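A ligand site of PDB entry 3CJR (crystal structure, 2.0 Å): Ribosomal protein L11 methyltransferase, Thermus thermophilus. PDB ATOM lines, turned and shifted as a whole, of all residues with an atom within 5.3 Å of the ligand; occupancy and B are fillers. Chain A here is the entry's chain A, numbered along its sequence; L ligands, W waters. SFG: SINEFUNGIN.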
ATOM      1  N   PHE A  99      13.755  21.572   9.358  1.00  0.00           N
ATOM      2  CA  PHE A  99      14.965  22.055  10.019  1.00  0.00           C
ATOM      3  C   PHE A  99      15.341  23.441   9.489  1.00  0.00           C
ATOM      4  O   PHE A  99      15.187  23.732   8.301  1.00  0.00           O
ATOM      5  CB  PHE A  99      16.131  21.078   9.796  1.00  0.00           C
ATOM      6  CG  PHE A  99      17.260  21.236  10.792  1.00  0.00           C
ATOM      7  CD1 PHE A  99      18.275  22.171  10.576  1.00  0.00           C
ATOM      8  CD2 PHE A  99      17.310  20.443  11.934  1.00  0.00           C
ATOM      9  CE1 PHE A  99      19.324  22.313  11.483  1.00  0.00           C
ATOM     10  CE2 PHE A  99      18.356  20.585  12.854  1.00  0.00           C
ATOM     11  CZ  PHE A  99      19.365  21.520  12.622  1.00  0.00           C
ATOM     12  N   GLY A 100      15.819  24.289  10.406  1.00  0.00           N
ATOM     13  CA  GLY A 100      16.201  25.646  10.081  1.00  0.00           C
ATOM     14  C   GLY A 100      15.484  26.662  10.936  1.00  0.00           C
ATOM     15  O   GLY A 100      15.261  27.796  10.509  1.00  0.00           O
ATOM     16  N   THR A 101      15.132  26.261  12.153  1.00  0.00           N
ATOM     17  CA  THR A 101      14.467  27.135  13.122  1.00  0.00           C
ATOM     18  C   THR A 101      15.376  28.308  13.484  1.00  0.00           C
ATOM     19  O   THR A 101      14.921  29.350  13.950  1.00  0.00           O
ATOM     20  CB  THR A 101      14.055  26.373  14.398  1.00  0.00           C
ATOM     21  OG1 THR A 101      13.404  25.155  14.036  1.00  0.00           O
ATOM     22  CG2 THR A 101      13.101  27.201  15.247  1.00  0.00           C
ATOM     23  N   THR A 107      23.147  25.745  12.206  1.00  0.00           N
ATOM     24  CA  THR A 107      22.497  26.855  11.522  1.00  0.00           C
ATOM     25  C   THR A 107      23.148  28.180  11.884  1.00  0.00           C
ATOM     26  O   THR A 107      23.419  29.015  11.010  1.00  0.00           O
ATOM     27  CB  THR A 107      20.996  26.910  11.860  1.00  0.00           C
ATOM     28  OG1 THR A 107      20.411  25.618  11.635  1.00  0.00           O
ATOM     29  CG2 THR A 107      20.279  27.954  10.998  1.00  0.00           C
ATOM     30  N   ASP A 126      22.439  27.349  -1.449  1.00  0.00           N
ATOM     31  CA  ASP A 126      22.141  26.806  -0.132  1.00  0.00           C
ATOM     32  C   ASP A 126      21.621  25.379  -0.328  1.00  0.00           C
ATOM     33  O   ASP A 126      20.447  25.170  -0.663  1.00  0.00           O
ATOM     34  CB  ASP A 126      21.135  27.712   0.606  1.00  0.00           C
ATOM     35  CG  ASP A 126      20.630  27.123   1.922  1.00  0.00           C
ATOM     36  OD1 ASP A 126      21.293  26.246   2.525  1.00  0.00           O
ATOM     37  OD2 ASP A 126      19.547  27.568   2.368  1.00  0.00           O
ATOM     38  N   LEU A 127      22.518  24.411  -0.168  1.00  0.00           N
ATOM     39  CA  LEU A 127      22.198  23.013  -0.416  1.00  0.00           C
ATOM     40  C   LEU A 127      21.524  22.393   0.799  1.00  0.00           C
ATOM     41  O   LEU A 127      22.137  22.261   1.859  1.00  0.00           O
ATOM     42  CB  LEU A 127      23.456  22.235  -0.819  1.00  0.00           C
ATOM     43  CG  LEU A 127      23.374  20.747  -1.143  1.00  0.00           C
ATOM     44  CD1 LEU A 127      22.518  20.484  -2.381  1.00  0.00           C
ATOM     45  CD2 LEU A 127      24.776  20.205  -1.348  1.00  0.00           C
ATOM     46  N   GLY A 128      20.267  22.002   0.617  1.00  0.00           N
ATOM     47  CA  GLY A 128      19.449  21.487   1.714  1.00  0.00           C
ATOM     48  C   GLY A 128      18.858  22.646   2.490  1.00  0.00           C
ATOM     49  O   GLY A 128      19.135  22.818   3.681  1.00  0.00           O
ATOM     50  N   THR A 129      18.030  23.442   1.806  1.00  0.00           N
ATOM     51  CA  THR A 129      17.569  24.720   2.332  1.00  0.00           C
ATOM     52  C   THR A 129      16.571  24.624   3.486  1.00  0.00           C
ATOM     53  O   THR A 129      16.511  25.532   4.328  1.00  0.00           O
ATOM     54  CB  THR A 129      17.039  25.646   1.203  1.00  0.00           C
ATOM     55  OG1 THR A 129      17.025  27.009   1.652  1.00  0.00           O
ATOM     56  CG2 THR A 129      15.635  25.225   0.722  1.00  0.00           C
ATOM     57  N   GLY A 130      15.800  23.544   3.529  1.00  0.00           N
ATOM     58  CA  GLY A 130      14.786  23.344   4.553  1.00  0.00           C
ATOM     59  C   GLY A 130      13.838  24.518   4.660  1.00  0.00           C
ATOM     60  O   GLY A 130      13.183  24.884   3.680  1.00  0.00           O
ATOM     61  N   SER A 131      13.784  25.123   5.854  1.00  0.00           N
ATOM     62  CA  SER A 131      12.991  26.314   6.151  1.00  0.00           C
ATOM     63  C   SER A 131      13.325  27.519   5.279  1.00  0.00           C
ATOM     64  O   SER A 131      12.539  28.464   5.169  1.00  0.00           O
ATOM     65  CB  SER A 131      13.204  26.719   7.623  1.00  0.00           C
ATOM     66  OG  SER A 131      14.519  27.231   7.823  1.00  0.00           O
ATOM     67  N   VAL A 133      16.136  29.372   5.823  1.00  0.00           N
ATOM     68  CA  VAL A 133      16.840  30.350   6.672  1.00  0.00           C
ATOM     69  C   VAL A 133      18.160  30.898   6.090  1.00  0.00           C
ATOM     70  O   VAL A 133      18.383  32.108   6.084  1.00  0.00           O
ATOM     71  CB  VAL A 133      17.017  29.832   8.149  1.00  0.00           C
ATOM     72  CG1 VAL A 133      17.943  28.610   8.202  1.00  0.00           C
ATOM     73  CG2 VAL A 133      17.504  30.949   9.076  1.00  0.00           C
ATOM     74  N   LEU A 134      19.013  30.015   5.576  1.00  0.00           N
ATOM     75  CA  LEU A 134      20.321  30.423   5.075  1.00  0.00           C
ATOM     76  C   LEU A 134      20.241  31.166   3.737  1.00  0.00           C
ATOM     77  O   LEU A 134      21.025  32.091   3.494  1.00  0.00           O
ATOM     78  CB  LEU A 134      21.285  29.233   4.986  1.00  0.00           C
ATOM     79  CG  LEU A 134      21.570  28.428   6.256  1.00  0.00           C
ATOM     80  CD1 LEU A 134      22.590  27.319   5.961  1.00  0.00           C
ATOM     81  CD2 LEU A 134      22.036  29.301   7.408  1.00  0.00           C
ATOM     82  N   VAL A 148      18.001  24.822  -2.569  1.00  0.00           N
ATOM     83  CA  VAL A 148      17.463  23.546  -3.081  1.00  0.00           C
ATOM     84  C   VAL A 148      17.251  22.538  -1.969  1.00  0.00           C
ATOM     85  O   VAL A 148      17.996  22.520  -0.974  1.00  0.00           O
ATOM     86  CB  VAL A 148      18.322  22.916  -4.227  1.00  0.00           C
ATOM     87  CG1 VAL A 148      18.449  23.871  -5.411  1.00  0.00           C
ATOM     88  CG2 VAL A 148      19.699  22.485  -3.732  1.00  0.00           C
ATOM     89  N   ASP A 149      16.233  21.695  -2.121  1.00  0.00           N
ATOM     90  CA  ASP A 149      15.951  20.634  -1.172  1.00  0.00           C
ATOM     91  C   ASP A 149      15.339  19.419  -1.868  1.00  0.00           C
ATOM     92  O   ASP A 149      14.461  19.566  -2.713  1.00  0.00           O
ATOM     93  CB  ASP A 149      15.021  21.138  -0.070  1.00  0.00           C
ATOM     94  CG  ASP A 149      15.203  20.399   1.237  1.00  0.00           C
ATOM     95  OD1 ASP A 149      15.632  21.036   2.220  1.00  0.00           O
ATOM     96  OD2 ASP A 149      14.938  19.178   1.282  1.00  0.00           O
ATOM     97  N   ILE A 150      15.821  18.231  -1.515  1.00  0.00           N
ATOM     98  CA  ILE A 150      15.286  16.980  -2.075  1.00  0.00           C
ATOM     99  C   ILE A 150      13.881  16.669  -1.563  1.00  0.00           C
ATOM    100  O   ILE A 150      13.157  15.863  -2.147  1.00  0.00           O
ATOM    101  CB  ILE A 150      16.222  15.766  -1.836  1.00  0.00           C
ATOM    102  CG1 ILE A 150      16.595  15.634  -0.348  1.00  0.00           C
ATOM    103  CG2 ILE A 150      17.471  15.861  -2.730  1.00  0.00           C
ATOM    104  CD1 ILE A 150      17.147  14.267   0.047  1.00  0.00           C
ATOM    105  N   ASP A 151      13.499  17.318  -0.455  1.00  0.00           N
ATOM    106  CA  ASP A 151      12.165  17.203   0.106  1.00  0.00           C
ATOM    107  C   ASP A 151      11.305  18.366  -0.381  1.00  0.00           C
ATOM    108  O   ASP A 151      11.489  19.507   0.060  1.00  0.00           O
ATOM    109  CB  ASP A 151      12.235  17.176   1.637  1.00  0.00           C
ATOM    110  CG  ASP A 151      10.874  16.990   2.296  1.00  0.00           C
ATOM    111  OD1 ASP A 151       9.854  16.833   1.587  1.00  0.00           O
ATOM    112  OD2 ASP A 151      10.824  16.995   3.547  1.00  0.00           O
ATOM    113  N   VAL A 154       9.168  21.064   2.132  1.00  0.00           N
ATOM    114  CA  VAL A 154       9.708  22.227   2.826  1.00  0.00           C
ATOM    115  C   VAL A 154       9.631  23.494   1.979  1.00  0.00           C
ATOM    116  O   VAL A 154       9.733  24.607   2.492  1.00  0.00           O
ATOM    117  CB  VAL A 154      11.183  22.012   3.306  1.00  0.00           C
ATOM    118  CG1 VAL A 154      11.305  20.753   4.144  1.00  0.00           C
ATOM    119  CG2 VAL A 154      12.145  21.981   2.132  1.00  0.00           C
ATOM    120  N   GLY A 174      15.269  19.415  -5.459  1.00  0.00           N
ATOM    121  CA  GLY A 174      16.423  18.686  -5.975  1.00  0.00           C
ATOM    122  C   GLY A 174      17.687  18.918  -5.171  1.00  0.00           C
ATOM    123  O   GLY A 174      17.631  19.327  -4.008  1.00  0.00           O
ATOM    124  N   SER A 175      18.823  18.659  -5.809  1.00  0.00           N
ATOM    125  CA  SER A 175      20.116  18.739  -5.149  1.00  0.00           C
ATOM    126  C   SER A 175      21.112  19.470  -6.063  1.00  0.00           C
ATOM    127  O   SER A 175      20.717  20.363  -6.813  1.00  0.00           O
ATOM    128  CB  SER A 175      20.611  17.326  -4.810  1.00  0.00           C
ATOM    129  OG  SER A 175      21.683  17.367  -3.876  1.00  0.00           O
ATOM    130  N   LEU A 176      22.388  19.090  -5.995  1.00  0.00           N
ATOM    131  CA  LEU A 176      23.447  19.700  -6.798  1.00  0.00           C
ATOM    132  C   LEU A 176      23.152  19.693  -8.305  1.00  0.00           C
ATOM    133  O   LEU A 176      23.417  20.679  -9.000  1.00  0.00           O
ATOM    134  CB  LEU A 176      24.794  19.016  -6.537  1.00  0.00           C
ATOM    135  CG  LEU A 176      25.911  19.723  -5.759  1.00  0.00           C
ATOM    136  CD1 LEU A 176      25.434  20.892  -4.907  1.00  0.00           C
ATOM    137  CD2 LEU A 176      26.688  18.703  -4.930  1.00  0.00           C
ATOM    138  N   ASN A 191      24.444  22.886   5.160  1.00  0.00           N
ATOM    139  CA  ASN A 191      24.257  22.316   6.490  1.00  0.00           C
ATOM    140  C   ASN A 191      23.671  20.920   6.345  1.00  0.00           C
ATOM    141  O   ASN A 191      22.448  20.735   6.343  1.00  0.00           O
ATOM    142  CB  ASN A 191      23.347  23.217   7.328  1.00  0.00           C
ATOM    143  CG  ASN A 191      23.231  22.759   8.781  1.00  0.00           C
ATOM    144  OD1 ASN A 191      23.882  21.797   9.198  1.00  0.00           O
ATOM    145  ND2 ASN A 191      22.402  23.454   9.551  1.00  0.00           N
ATOM    146  N   LEU A 192      24.559  19.947   6.194  1.00  0.00           N
ATOM    147  CA  LEU A 192      24.147  18.572   5.981  1.00  0.00           C
ATOM    148  C   LEU A 192      24.755  17.674   7.052  1.00  0.00           C
ATOM    149  O   LEU A 192      24.453  17.843   8.240  1.00  0.00           O
ATOM    150  CB  LEU A 192      24.511  18.117   4.559  1.00  0.00           C
ATOM    151  CG  LEU A 192      23.918  18.923   3.396  1.00  0.00           C
ATOM    152  CD1 LEU A 192      24.519  18.494   2.056  1.00  0.00           C
ATOM    153  CD2 LEU A 192      22.396  18.836   3.350  1.00  0.00           C
ATOM    154  N   LEU A 196      27.953  12.875   3.854  1.00  0.00           N
ATOM    155  CA  LEU A 196      27.400  13.426   2.616  1.00  0.00           C
ATOM    156  C   LEU A 196      28.357  14.452   2.002  1.00  0.00           C
ATOM    157  O   LEU A 196      28.601  14.418   0.801  1.00  0.00           O
ATOM    158  CB  LEU A 196      26.011  14.015   2.850  1.00  0.00           C
ATOM    159  CG  LEU A 196      25.141  14.381   1.635  1.00  0.00           C
ATOM    160  CD1 LEU A 196      25.045  13.257   0.602  1.00  0.00           C
ATOM    161  CD2 LEU A 196      23.757  14.803   2.115  1.00  0.00           C
ATOM    162  N   LEU A 200      30.144  14.199  -1.714  1.00  0.00           N
ATOM    163  CA  LEU A 200      29.779  15.262  -2.648  1.00  0.00           C
ATOM    164  C   LEU A 200      30.919  16.229  -2.982  1.00  0.00           C
ATOM    165  O   LEU A 200      30.792  17.059  -3.877  1.00  0.00           O
ATOM    166  CB  LEU A 200      28.600  16.057  -2.076  1.00  0.00           C
ATOM    167  CG  LEU A 200      27.167  15.834  -2.564  1.00  0.00           C
ATOM    168  CD1 LEU A 200      26.879  14.401  -3.005  1.00  0.00           C
ATOM    169  CD2 LEU A 200      26.187  16.299  -1.508  1.00  0.00           C
HETATM  170  N   SFG L   1      19.605  24.686   5.669  1.00  0.00           N
HETATM  171  CA  SFG L   1      18.887  24.534   6.975  1.00  0.00           C
HETATM  172  C   SFG L   1      19.741  24.951   8.145  1.00  0.00           C
HETATM  173  O   SFG L   1      20.920  25.252   8.004  1.00  0.00           O
HETATM  174  OXT SFG L   1      19.266  25.014   9.284  1.00  0.00           O
HETATM  175  CB  SFG L   1      18.341  23.108   7.140  1.00  0.00           C
HETATM  176  CG  SFG L   1      19.366  21.989   6.978  1.00  0.00           C
HETATM  177  CD  SFG L   1      18.716  20.626   7.223  1.00  0.00           C
HETATM  178  NE  SFG L   1      19.215  20.081   8.469  1.00  0.00           N
HETATM  179  C5' SFG L   1      19.064  19.636   6.122  1.00  0.00           C
HETATM  180  C4' SFG L   1      18.092  19.679   4.935  1.00  0.00           C
HETATM  181  O4' SFG L   1      18.786  19.202   3.786  1.00  0.00           O
HETATM  182  C3' SFG L   1      16.858  18.802   5.081  1.00  0.00           C
HETATM  183  O3' SFG L   1      15.709  19.633   4.893  1.00  0.00           O
HETATM  184  C2' SFG L   1      16.949  17.773   3.974  1.00  0.00           C
HETATM  185  O2' SFG L   1      15.680  17.578   3.341  1.00  0.00           O
HETATM  186  C1' SFG L   1      17.924  18.395   2.987  1.00  0.00           C
HETATM  187  N9  SFG L   1      18.791  17.428   2.265  1.00  0.00           N
HETATM  188  C8  SFG L   1      19.311  16.282   2.742  1.00  0.00           C
HETATM  189  N7  SFG L   1      20.079  15.669   1.815  1.00  0.00           N
HETATM  190  C5  SFG L   1      20.072  16.439   0.706  1.00  0.00           C
HETATM  191  C6  SFG L   1      20.686  16.386  -0.638  1.00  0.00           C
HETATM  192  N6  SFG L   1      21.477  15.349  -1.005  1.00  0.00           N
HETATM  193  N1  SFG L   1      20.425  17.410  -1.496  1.00  0.00           N
HETATM  194  C2  SFG L   1      19.637  18.448  -1.143  1.00  0.00           C
HETATM  195  N3  SFG L   1      19.052  18.561   0.059  1.00  0.00           N
HETATM  196  C4  SFG L   1      19.236  17.607   1.011  1.00  0.00           C
HETATM  197  O   HOH W   1      21.293  12.512  -0.088  1.00  0.00           O
HETATM  198  O   HOH W   2      22.310  14.223  -3.506  1.00  0.00           O
HETATM  199  O   HOH W   3      22.002  24.039   4.050  1.00  0.00           O
HETATM  200  O   HOH W   4      14.794  14.796   3.064  1.00  0.00           O
HETATM  201  O   HOH W   5      18.985  15.626   6.144  1.00  0.00           O
HETATM  202  O   HOH W   6      20.567  13.115   2.893  1.00  0.00           O
HETATM  203  O   HOH W   7      18.596  27.130   4.794  1.00  0.00           O
HETATM  204  O   HOH W   8      21.597  19.115   8.578  1.00  0.00           O
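Phe 99 touches the ligand. CA of Gly 100 touches OXT of the ligand, at 3.2 Å. Leu 127 touches the ligand (CD1 to C2, 3.7 Å). CA of Gly 130 touches O3' of the ligand, 3.8 Å away. Val 133 touches the ligand. Leu 134 touches the ligand (CD1 to O, 3.4 Å). Ile 150 touches the ligand. Asp 151 touches the ligand. O of Gly 174 touches C2 of the ligand (3.6 Å). CD2 of Leu 192 touches O4' of the ligand, 3.7 Å away. Leu 196 touches the ligand (CD2 to N7, 3.8 Å). Of the 24 residues printed, 18 come within 4 Å of the ligand. Along chain A the residues within 4 Å of the ligand span positions 99 to 196. The nearest printed residue that does not touch the ligand is Val 148 (4.2 Å).
Water W8 lies within hydrogen-bond range of a nitrogen (NE) of the ligand (2.6 Å), the backbone carbonyl oxygen (O) of Asn 191 (2.9 Å) and the backbone carbonyl oxygen (O) of Leu 192 (3.1 Å). Water W7 lies within hydrogen-bond range of OD2 of Asp 126, O of Thr 129, N of the ligand, N of Leu 134 and N of Val 133. Water W2 lies within hydrogen-bond range of a nitrogen (N6) of the ligand (2.9 Å) and the side-chain hydroxyl of Ser 175 (3.2 Å).
OD1 of Asp 149 is in hydrogen-bond range of N of Thr 129, 3.4 Å away. N of Ile 150 is in hydrogen-bond range of O of Gly 174. The backbone NH of Gly 174 lies within hydrogen-bond range of the backbone carbonyl oxygen of Asp 149 (2.9 Å). O of Val 148 sits at hydrogen-bond distance from N of Thr 129, 2.9 Å away. O of Phe 99 sits at hydrogen-bond distance from N of Ser 131. The backbone carbonyl oxygen (O) of Val 148 lies within hydrogen-bond range of the backbone NH (N) of Gly 128 (2.8 Å). The backbone NH (N) of Val 133 is in hydrogen-bond range of the side-chain hydroxyl (OG) of Ser 131, 3.3 Å away. OG1 of Thr 129 sits at hydrogen-bond distance from OD2 of Asp 126 (2.7 Å).
ND2 of Asn 191 sits at hydrogen-bond distance from O of the ligand, at 2.8 Å. The side-chain carboxylate (OD2) of Asp 149 sits at hydrogen-bond distance from an oxygen (O2') of the ligand (2.7 Å). The side-chain carboxylate (OD1) of Asp 126 is in salt-bridge range of a nitrogen (N) of the ligand (3.9 Å). OG1 of Thr 107 sits at hydrogen-bond distance from OXT of the ligand. The backbone carbonyl oxygen (O) of Thr 129 lies within hydrogen-bond range of a nitrogen (N) of the ligand (3.5 Å). N1 of the ligand lies within hydrogen-bond range of OG of Ser 175 (2.7 Å). N of the ligand lies within hydrogen-bond range of O of Gly 128 (2.8 Å).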
